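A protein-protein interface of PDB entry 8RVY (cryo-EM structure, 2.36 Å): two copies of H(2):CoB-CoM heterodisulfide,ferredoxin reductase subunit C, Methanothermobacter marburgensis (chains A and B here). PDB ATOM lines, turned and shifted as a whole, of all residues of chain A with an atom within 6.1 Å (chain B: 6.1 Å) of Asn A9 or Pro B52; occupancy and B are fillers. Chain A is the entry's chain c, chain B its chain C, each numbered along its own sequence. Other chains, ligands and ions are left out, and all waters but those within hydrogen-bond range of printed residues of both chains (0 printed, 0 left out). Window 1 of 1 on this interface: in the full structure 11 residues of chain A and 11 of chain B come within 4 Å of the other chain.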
ATOM      1  N   LEU A   3      -5.392 -32.216 -33.651  1.00  0.00           N
ATOM      2  CA  LEU A   3      -5.653 -30.955 -32.975  1.00  0.00           C
ATOM      3  C   LEU A   3      -4.532 -29.945 -33.158  1.00  0.00           C
ATOM      4  O   LEU A   3      -4.658 -28.811 -32.692  1.00  0.00           O
ATOM      5  CB  LEU A   3      -5.879 -31.198 -31.481  1.00  0.00           C
ATOM      6  CG  LEU A   3      -7.221 -31.820 -31.107  1.00  0.00           C
ATOM      7  CD1 LEU A   3      -7.261 -32.118 -29.622  1.00  0.00           C
ATOM      8  CD2 LEU A   3      -8.372 -30.912 -31.501  1.00  0.00           C
ATOM      9  N   LEU A   4      -3.446 -30.322 -33.827  1.00  0.00           N
ATOM     10  CA  LEU A   4      -2.338 -29.402 -34.024  1.00  0.00           C
ATOM     11  C   LEU A   4      -2.787 -28.209 -34.853  1.00  0.00           C
ATOM     12  O   LEU A   4      -3.267 -28.366 -35.980  1.00  0.00           O
ATOM     13  CB  LEU A   4      -1.175 -30.118 -34.712  1.00  0.00           C
ATOM     14  CG  LEU A   4       0.003 -29.231 -35.127  1.00  0.00           C
ATOM     15  CD1 LEU A   4       0.654 -28.614 -33.908  1.00  0.00           C
ATOM     16  CD2 LEU A   4       1.017 -30.013 -35.936  1.00  0.00           C
ATOM     17  N   GLN A   5      -2.635 -27.013 -34.290  1.00  0.00           N
ATOM     18  CA  GLN A   5      -2.821 -25.777 -35.044  1.00  0.00           C
ATOM     19  C   GLN A   5      -1.834 -24.767 -34.473  1.00  0.00           C
ATOM     20  O   GLN A   5      -2.062 -24.204 -33.399  1.00  0.00           O
ATOM     21  CB  GLN A   5      -4.254 -25.275 -34.967  1.00  0.00           C
ATOM     22  CG  GLN A   5      -4.453 -23.908 -35.599  1.00  0.00           C
ATOM     23  CD  GLN A   5      -4.362 -23.937 -37.107  1.00  0.00           C
ATOM     24  OE1 GLN A   5      -3.364 -23.513 -37.686  1.00  0.00           O
ATOM     25  NE2 GLN A   5      -5.404 -24.440 -37.752  1.00  0.00           N
ATOM     26  N   ARG A   6      -0.750 -24.540 -35.205  1.00  0.00           N
ATOM     27  CA  ARG A   6       0.371 -23.759 -34.712  1.00  0.00           C
ATOM     28  C   ARG A   6       0.139 -22.256 -34.779  1.00  0.00           C
ATOM     29  O   ARG A   6       0.955 -21.502 -34.242  1.00  0.00           O
ATOM     30  CB  ARG A   6       1.617 -24.127 -35.514  1.00  0.00           C
ATOM     31  CG  ARG A   6       2.916 -24.096 -34.729  1.00  0.00           C
ATOM     32  CD  ARG A   6       4.169 -24.538 -35.519  1.00  0.00           C
ATOM     33  NE  ARG A   6       4.055 -25.834 -36.186  1.00  0.00           N
ATOM     34  CZ  ARG A   6       3.310 -26.093 -37.254  1.00  0.00           C
ATOM     35  NH1 ARG A   6       2.726 -25.128 -37.944  1.00  0.00           N
ATOM     36  NH2 ARG A   6       3.175 -27.351 -37.657  1.00  0.00           N
ATOM     37  N   GLU A   7      -0.944 -21.802 -35.409  1.00  0.00           N
ATOM     38  CA  GLU A   7      -1.156 -20.381 -35.648  1.00  0.00           C
ATOM     39  C   GLU A   7      -2.320 -19.775 -34.879  1.00  0.00           C
ATOM     40  O   GLU A   7      -2.261 -18.588 -34.556  1.00  0.00           O
ATOM     41  CB  GLU A   7      -1.375 -20.122 -37.144  1.00  0.00           C
ATOM     42  CG  GLU A   7      -0.255 -20.632 -38.036  1.00  0.00           C
ATOM     43  CD  GLU A   7       1.021 -19.824 -37.891  1.00  0.00           C
ATOM     44  OE1 GLU A   7       2.109 -20.433 -37.824  1.00  0.00           O
ATOM     45  OE2 GLU A   7       0.936 -18.578 -37.842  1.00  0.00           O
ATOM     46  N   GLU A   8      -3.375 -20.532 -34.579  1.00  0.00           N
ATOM     47  CA  GLU A   8      -4.542 -19.949 -33.929  1.00  0.00           C
ATOM     48  C   GLU A   8      -4.481 -20.019 -32.411  1.00  0.00           C
ATOM     49  O   GLU A   8      -5.427 -19.578 -31.752  1.00  0.00           O
ATOM     50  CB  GLU A   8      -5.837 -20.628 -34.403  1.00  0.00           C
ATOM     51  CG  GLU A   8      -6.379 -21.702 -33.458  1.00  0.00           C
ATOM     52  CD  GLU A   8      -7.310 -22.682 -34.141  1.00  0.00           C
ATOM     53  OE1 GLU A   8      -7.671 -23.699 -33.510  1.00  0.00           O
ATOM     54  OE2 GLU A   8      -7.679 -22.441 -35.309  1.00  0.00           O
ATOM     55  N   ASN A   9      -3.406 -20.557 -31.837  1.00  0.00           N
ATOM     56  CA  ASN A   9      -3.329 -20.775 -30.398  1.00  0.00           C
ATOM     57  C   ASN A   9      -2.202 -19.991 -29.740  1.00  0.00           C
ATOM     58  O   ASN A   9      -1.855 -20.276 -28.590  1.00  0.00           O
ATOM     59  CB  ASN A   9      -3.170 -22.268 -30.104  1.00  0.00           C
ATOM     60  CG  ASN A   9      -4.412 -23.058 -30.442  1.00  0.00           C
ATOM     61  OD1 ASN A   9      -5.430 -22.952 -29.763  1.00  0.00           O
ATOM     62  ND2 ASN A   9      -4.340 -23.848 -31.502  1.00  0.00           N
ATOM     63  N   ILE A  10      -1.629 -19.011 -30.429  1.00  0.00           N
ATOM     64  CA  ILE A  10      -0.584 -18.171 -29.857  1.00  0.00           C
ATOM     65  C   ILE A  10      -0.673 -16.801 -30.509  1.00  0.00           C
ATOM     66  O   ILE A  10      -0.963 -16.688 -31.703  1.00  0.00           O
ATOM     67  CB  ILE A  10       0.812 -18.800 -30.049  1.00  0.00           C
ATOM     68  CG1 ILE A  10       1.837 -18.120 -29.144  1.00  0.00           C
ATOM     69  CG2 ILE A  10       1.245 -18.710 -31.502  1.00  0.00           C
ATOM     70  CD1 ILE A  10       2.921 -19.040 -28.675  1.00  0.00           C
ATOM     71  N   ILE A  11      -0.427 -15.759 -29.724  1.00  0.00           N
ATOM     72  CA  ILE A  11      -0.472 -14.383 -30.201  1.00  0.00           C
ATOM     73  C   ILE A  11       0.947 -13.835 -30.199  1.00  0.00           C
ATOM     74  O   ILE A  11       1.603 -13.790 -29.152  1.00  0.00           O
ATOM     75  CB  ILE A  11      -1.397 -13.507 -29.343  1.00  0.00           C
ATOM     76  CG1 ILE A  11      -2.833 -14.020 -29.407  1.00  0.00           C
ATOM     77  CG2 ILE A  11      -1.355 -12.072 -29.817  1.00  0.00           C
ATOM     78  CD1 ILE A  11      -3.633 -13.721 -28.169  1.00  0.00           C
ATOM     79  N   SER B  47       1.970 -27.837 -24.890  1.00  0.00           N
ATOM     80  CA  SER B  47       0.820 -28.260 -25.681  1.00  0.00           C
ATOM     81  C   SER B  47      -0.130 -27.099 -25.937  1.00  0.00           C
ATOM     82  O   SER B  47      -0.666 -26.960 -27.041  1.00  0.00           O
ATOM     83  CB  SER B  47       0.086 -29.396 -24.975  1.00  0.00           C
ATOM     84  OG  SER B  47       0.896 -30.550 -24.891  1.00  0.00           O
ATOM     85  N   GLY B  48      -0.346 -26.250 -24.933  1.00  0.00           N
ATOM     86  CA  GLY B  48      -1.243 -25.123 -25.093  1.00  0.00           C
ATOM     87  C   GLY B  48      -0.792 -24.122 -26.134  1.00  0.00           C
ATOM     88  O   GLY B  48      -1.602 -23.309 -26.588  1.00  0.00           O
ATOM     89  N   ARG B  49       0.481 -24.156 -26.523  1.00  0.00           N
ATOM     90  CA  ARG B  49       0.983 -23.250 -27.547  1.00  0.00           C
ATOM     91  C   ARG B  49       0.582 -23.668 -28.952  1.00  0.00           C
ATOM     92  O   ARG B  49       0.623 -22.836 -29.864  1.00  0.00           O
ATOM     93  CB  ARG B  49       2.507 -23.167 -27.475  1.00  0.00           C
ATOM     94  CG  ARG B  49       3.036 -22.334 -26.336  1.00  0.00           C
ATOM     95  CD  ARG B  49       4.409 -21.773 -26.652  1.00  0.00           C
ATOM     96  NE  ARG B  49       5.433 -22.804 -26.768  1.00  0.00           N
ATOM     97  CZ  ARG B  49       6.022 -23.398 -25.739  1.00  0.00           C
ATOM     98  NH1 ARG B  49       5.671 -23.134 -24.492  1.00  0.00           N
ATOM     99  NH2 ARG B  49       6.988 -24.280 -25.967  1.00  0.00           N
ATOM    100  N   ARG B  50       0.204 -24.929 -29.151  1.00  0.00           N
ATOM    101  CA  ARG B  50      -0.071 -25.454 -30.479  1.00  0.00           C
ATOM    102  C   ARG B  50      -1.374 -26.233 -30.568  1.00  0.00           C
ATOM    103  O   ARG B  50      -1.675 -26.775 -31.634  1.00  0.00           O
ATOM    104  CB  ARG B  50       1.083 -26.356 -30.941  1.00  0.00           C
ATOM    105  CG  ARG B  50       1.334 -27.555 -30.042  1.00  0.00           C
ATOM    106  CD  ARG B  50       2.746 -28.075 -30.199  1.00  0.00           C
ATOM    107  NE  ARG B  50       3.644 -27.499 -29.205  1.00  0.00           N
ATOM    108  CZ  ARG B  50       4.850 -27.010 -29.458  1.00  0.00           C
ATOM    109  NH1 ARG B  50       5.356 -27.000 -30.680  1.00  0.00           N
ATOM    110  NH2 ARG B  50       5.570 -26.517 -28.456  1.00  0.00           N
ATOM    111  N   THR B  51      -2.144 -26.311 -29.496  1.00  0.00           N
ATOM    112  CA  THR B  51      -3.438 -26.974 -29.493  1.00  0.00           C
ATOM    113  C   THR B  51      -4.399 -26.122 -28.685  1.00  0.00           C
ATOM    114  O   THR B  51      -3.973 -25.243 -27.929  1.00  0.00           O
ATOM    115  CB  THR B  51      -3.364 -28.385 -28.893  1.00  0.00           C
ATOM    116  OG1 THR B  51      -3.374 -28.301 -27.465  1.00  0.00           O
ATOM    117  CG2 THR B  51      -2.107 -29.104 -29.344  1.00  0.00           C
ATOM    118  N   PRO B  52      -5.705 -26.351 -28.826  1.00  0.00           N
ATOM    119  CA  PRO B  52      -6.678 -25.667 -27.967  1.00  0.00           C
ATOM    120  C   PRO B  52      -6.718 -26.176 -26.534  1.00  0.00           C
ATOM    121  O   PRO B  52      -7.643 -25.823 -25.800  1.00  0.00           O
ATOM    122  CB  PRO B  52      -8.012 -25.937 -28.680  1.00  0.00           C
ATOM    123  CG  PRO B  52      -7.792 -27.152 -29.465  1.00  0.00           C
ATOM    124  CD  PRO B  52      -6.358 -27.162 -29.865  1.00  0.00           C
ATOM    125  N   TYR B  53      -5.751 -26.997 -26.133  1.00  0.00           N
ATOM    126  CA  TYR B  53      -5.652 -27.450 -24.754  1.00  0.00           C
ATOM    127  C   TYR B  53      -5.309 -26.281 -23.840  1.00  0.00           C
ATOM    128  O   TYR B  53      -4.396 -25.504 -24.128  1.00  0.00           O
ATOM    129  CB  TYR B  53      -4.588 -28.542 -24.652  1.00  0.00           C
ATOM    130  CG  TYR B  53      -4.323 -29.049 -23.256  1.00  0.00           C
ATOM    131  CD1 TYR B  53      -5.354 -29.517 -22.458  1.00  0.00           C
ATOM    132  CD2 TYR B  53      -3.036 -29.070 -22.742  1.00  0.00           C
ATOM    133  CE1 TYR B  53      -5.112 -29.984 -21.186  1.00  0.00           C
ATOM    134  CE2 TYR B  53      -2.787 -29.534 -21.473  1.00  0.00           C
ATOM    135  CZ  TYR B  53      -3.827 -29.990 -20.700  1.00  0.00           C
ATOM    136  OH  TYR B  53      -3.582 -30.453 -19.433  1.00  0.00           O
ATOM    137  N   ARG B  54      -6.044 -26.157 -22.736  1.00  0.00           N
ATOM    138  CA  ARG B  54      -5.838 -25.080 -21.765  1.00  0.00           C
ATOM    139  C   ARG B  54      -5.927 -25.695 -20.372  1.00  0.00           C
ATOM    140  O   ARG B  54      -7.023 -25.952 -19.872  1.00  0.00           O
ATOM    141  CB  ARG B  54      -6.862 -23.966 -21.943  1.00  0.00           C
ATOM    142  CG  ARG B  54      -6.901 -23.362 -23.336  1.00  0.00           C
ATOM    143  CD  ARG B  54      -5.764 -22.385 -23.558  1.00  0.00           C
ATOM    144  NE  ARG B  54      -5.854 -21.736 -24.860  1.00  0.00           N
ATOM    145  CZ  ARG B  54      -5.361 -22.230 -25.986  1.00  0.00           C
ATOM    146  NH1 ARG B  54      -4.723 -23.387 -26.016  1.00  0.00           N
ATOM    147  NH2 ARG B  54      -5.514 -21.546 -27.115  1.00  0.00           N
ATOM    148  N   GLN B  57      -8.052 -23.871 -17.645  1.00  0.00           N
ATOM    149  CA  GLN B  57      -9.488 -24.075 -17.758  1.00  0.00           C
ATOM    150  C   GLN B  57      -9.887 -25.477 -17.320  1.00  0.00           C
ATOM    151  O   GLN B  57     -10.983 -25.664 -16.787  1.00  0.00           O
ATOM    152  CB  GLN B  57      -9.943 -23.802 -19.188  1.00  0.00           C
ATOM    153  CG  GLN B  57     -10.151 -22.326 -19.479  1.00  0.00           C
ATOM    154  CD  GLN B  57      -9.974 -21.987 -20.943  1.00  0.00           C
ATOM    155  OE1 GLN B  57      -9.334 -20.994 -21.290  1.00  0.00           O
ATOM    156  NE2 GLN B  57     -10.541 -22.812 -21.815  1.00  0.00           N
ATOM    157  N   THR B  75      -9.105 -32.454 -26.013  1.00  0.00           N
ATOM    158  CA  THR B  75      -7.889 -31.746 -25.640  1.00  0.00           C
ATOM    159  C   THR B  75      -7.352 -32.203 -24.295  1.00  0.00           C
ATOM    160  O   THR B  75      -6.196 -31.912 -23.976  1.00  0.00           O
ATOM    161  CB  THR B  75      -8.133 -30.235 -25.605  1.00  0.00           C
ATOM    162  OG1 THR B  75      -9.168 -29.934 -24.664  1.00  0.00           O
ATOM    163  CG2 THR B  75      -8.528 -29.720 -26.973  1.00  0.00           C
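N of Gln A5 is in hydrogen-bond range of O of Arg B50, 2.8 Å away. The side-chain amide oxygen of Asn A9 lies close to the backbone carbonyl oxygen of Thr B51, at 3.3 Å. The guanidinium group (NH2) of Arg B54 sits at hydrogen-bond distance from the side-chain amide oxygen (OD1) of Asn A9.
O of Gln A5 sits at hydrogen-bond distance from ND2 of Asn A9 (3.0 Å). O of Ser B47 is in hydrogen-bond range of OG1 of Thr B51 (3.1 Å). The backbone carbonyl oxygen of Gly B48 sits at hydrogen-bond distance from the guanidinium group of Arg B54, at 3.2 Å. The backbone NH (N) of Tyr B53 sits close to the side-chain hydroxyl (OG1) of Thr B51 (3.0 Å). The backbone carbonyl oxygen (O) of Thr B51 sits at hydrogen-bond distance from the guanidinium group (NH1) of Arg B54, at 2.8 Å.
Arg B50 touches Leu A3. O of Leu A3 touches CA of Thr B51, 3.9 Å away. Leu A3 touches Pro B52 (O to CD, 3.7 Å). Leu A3 touches Thr B75. Arg B50 touches Leu A4 (O to CA, 3.6 Å). Asn A9 touches Gly B48 (O to O, 3.6 Å). Arg B49 touches Asn A9. Asn A9 touches Arg B50. Asn A9 touches Pro B52 (OD1 to CA, 3.5 Å). Ile A10 touches Arg B49.
Printed residues of chain B within 4 Å of Asn A9: Gly B48 (3.6 Å), Arg B49 (3.8 Å), Arg B50 (3.9 Å), Thr B51 (3.3 Å), Pro B52 (3.5 Å) and Arg B54 (3.0 Å). Of chain A, only Leu A3 and Asn A9 come within 4 Å of Pro B52. Of the printed residues of chain A, Thr B75 touches Leu A3. Of the printed residues of chain B, Leu A3 touches Arg B50, Thr B51, Pro B52 and Thr B75. Printed residues of chain A within 4 Å of Arg B50: Leu A3, Leu A4, Gln A5 and Asn A9. Of the printed residues of chain B, Gln A5 touches Arg B50. Glu A8 touches none of the printed residues of chain B. The nearest residue of chain B that does not touch Asn A9 is Tyr B53 (5.4 Å). The nearest residue of chain A that does not touch Pro B52 is Glu A8 (5.2 Å).
Printed residues of chain A that touch a printed residue of chain B: Leu A3, Leu A4, Gln A5, Asn A9 and Ile A10. Hydrophobic or aromatic side chains of chain A within 4 Å of the printed part of chain B: Leu A3, Leu A4 and Ile A10. Printed residues of chain B that touch a printed residue of chain A: Gly B48, Arg B49, Arg B50, Thr B51, Pro B52, Arg B54 and Thr B75.
No position is printed for both chains. Of the 13 pairs that touch across the chains among the printed residues, none has its exchanged pair printed and touching as well.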
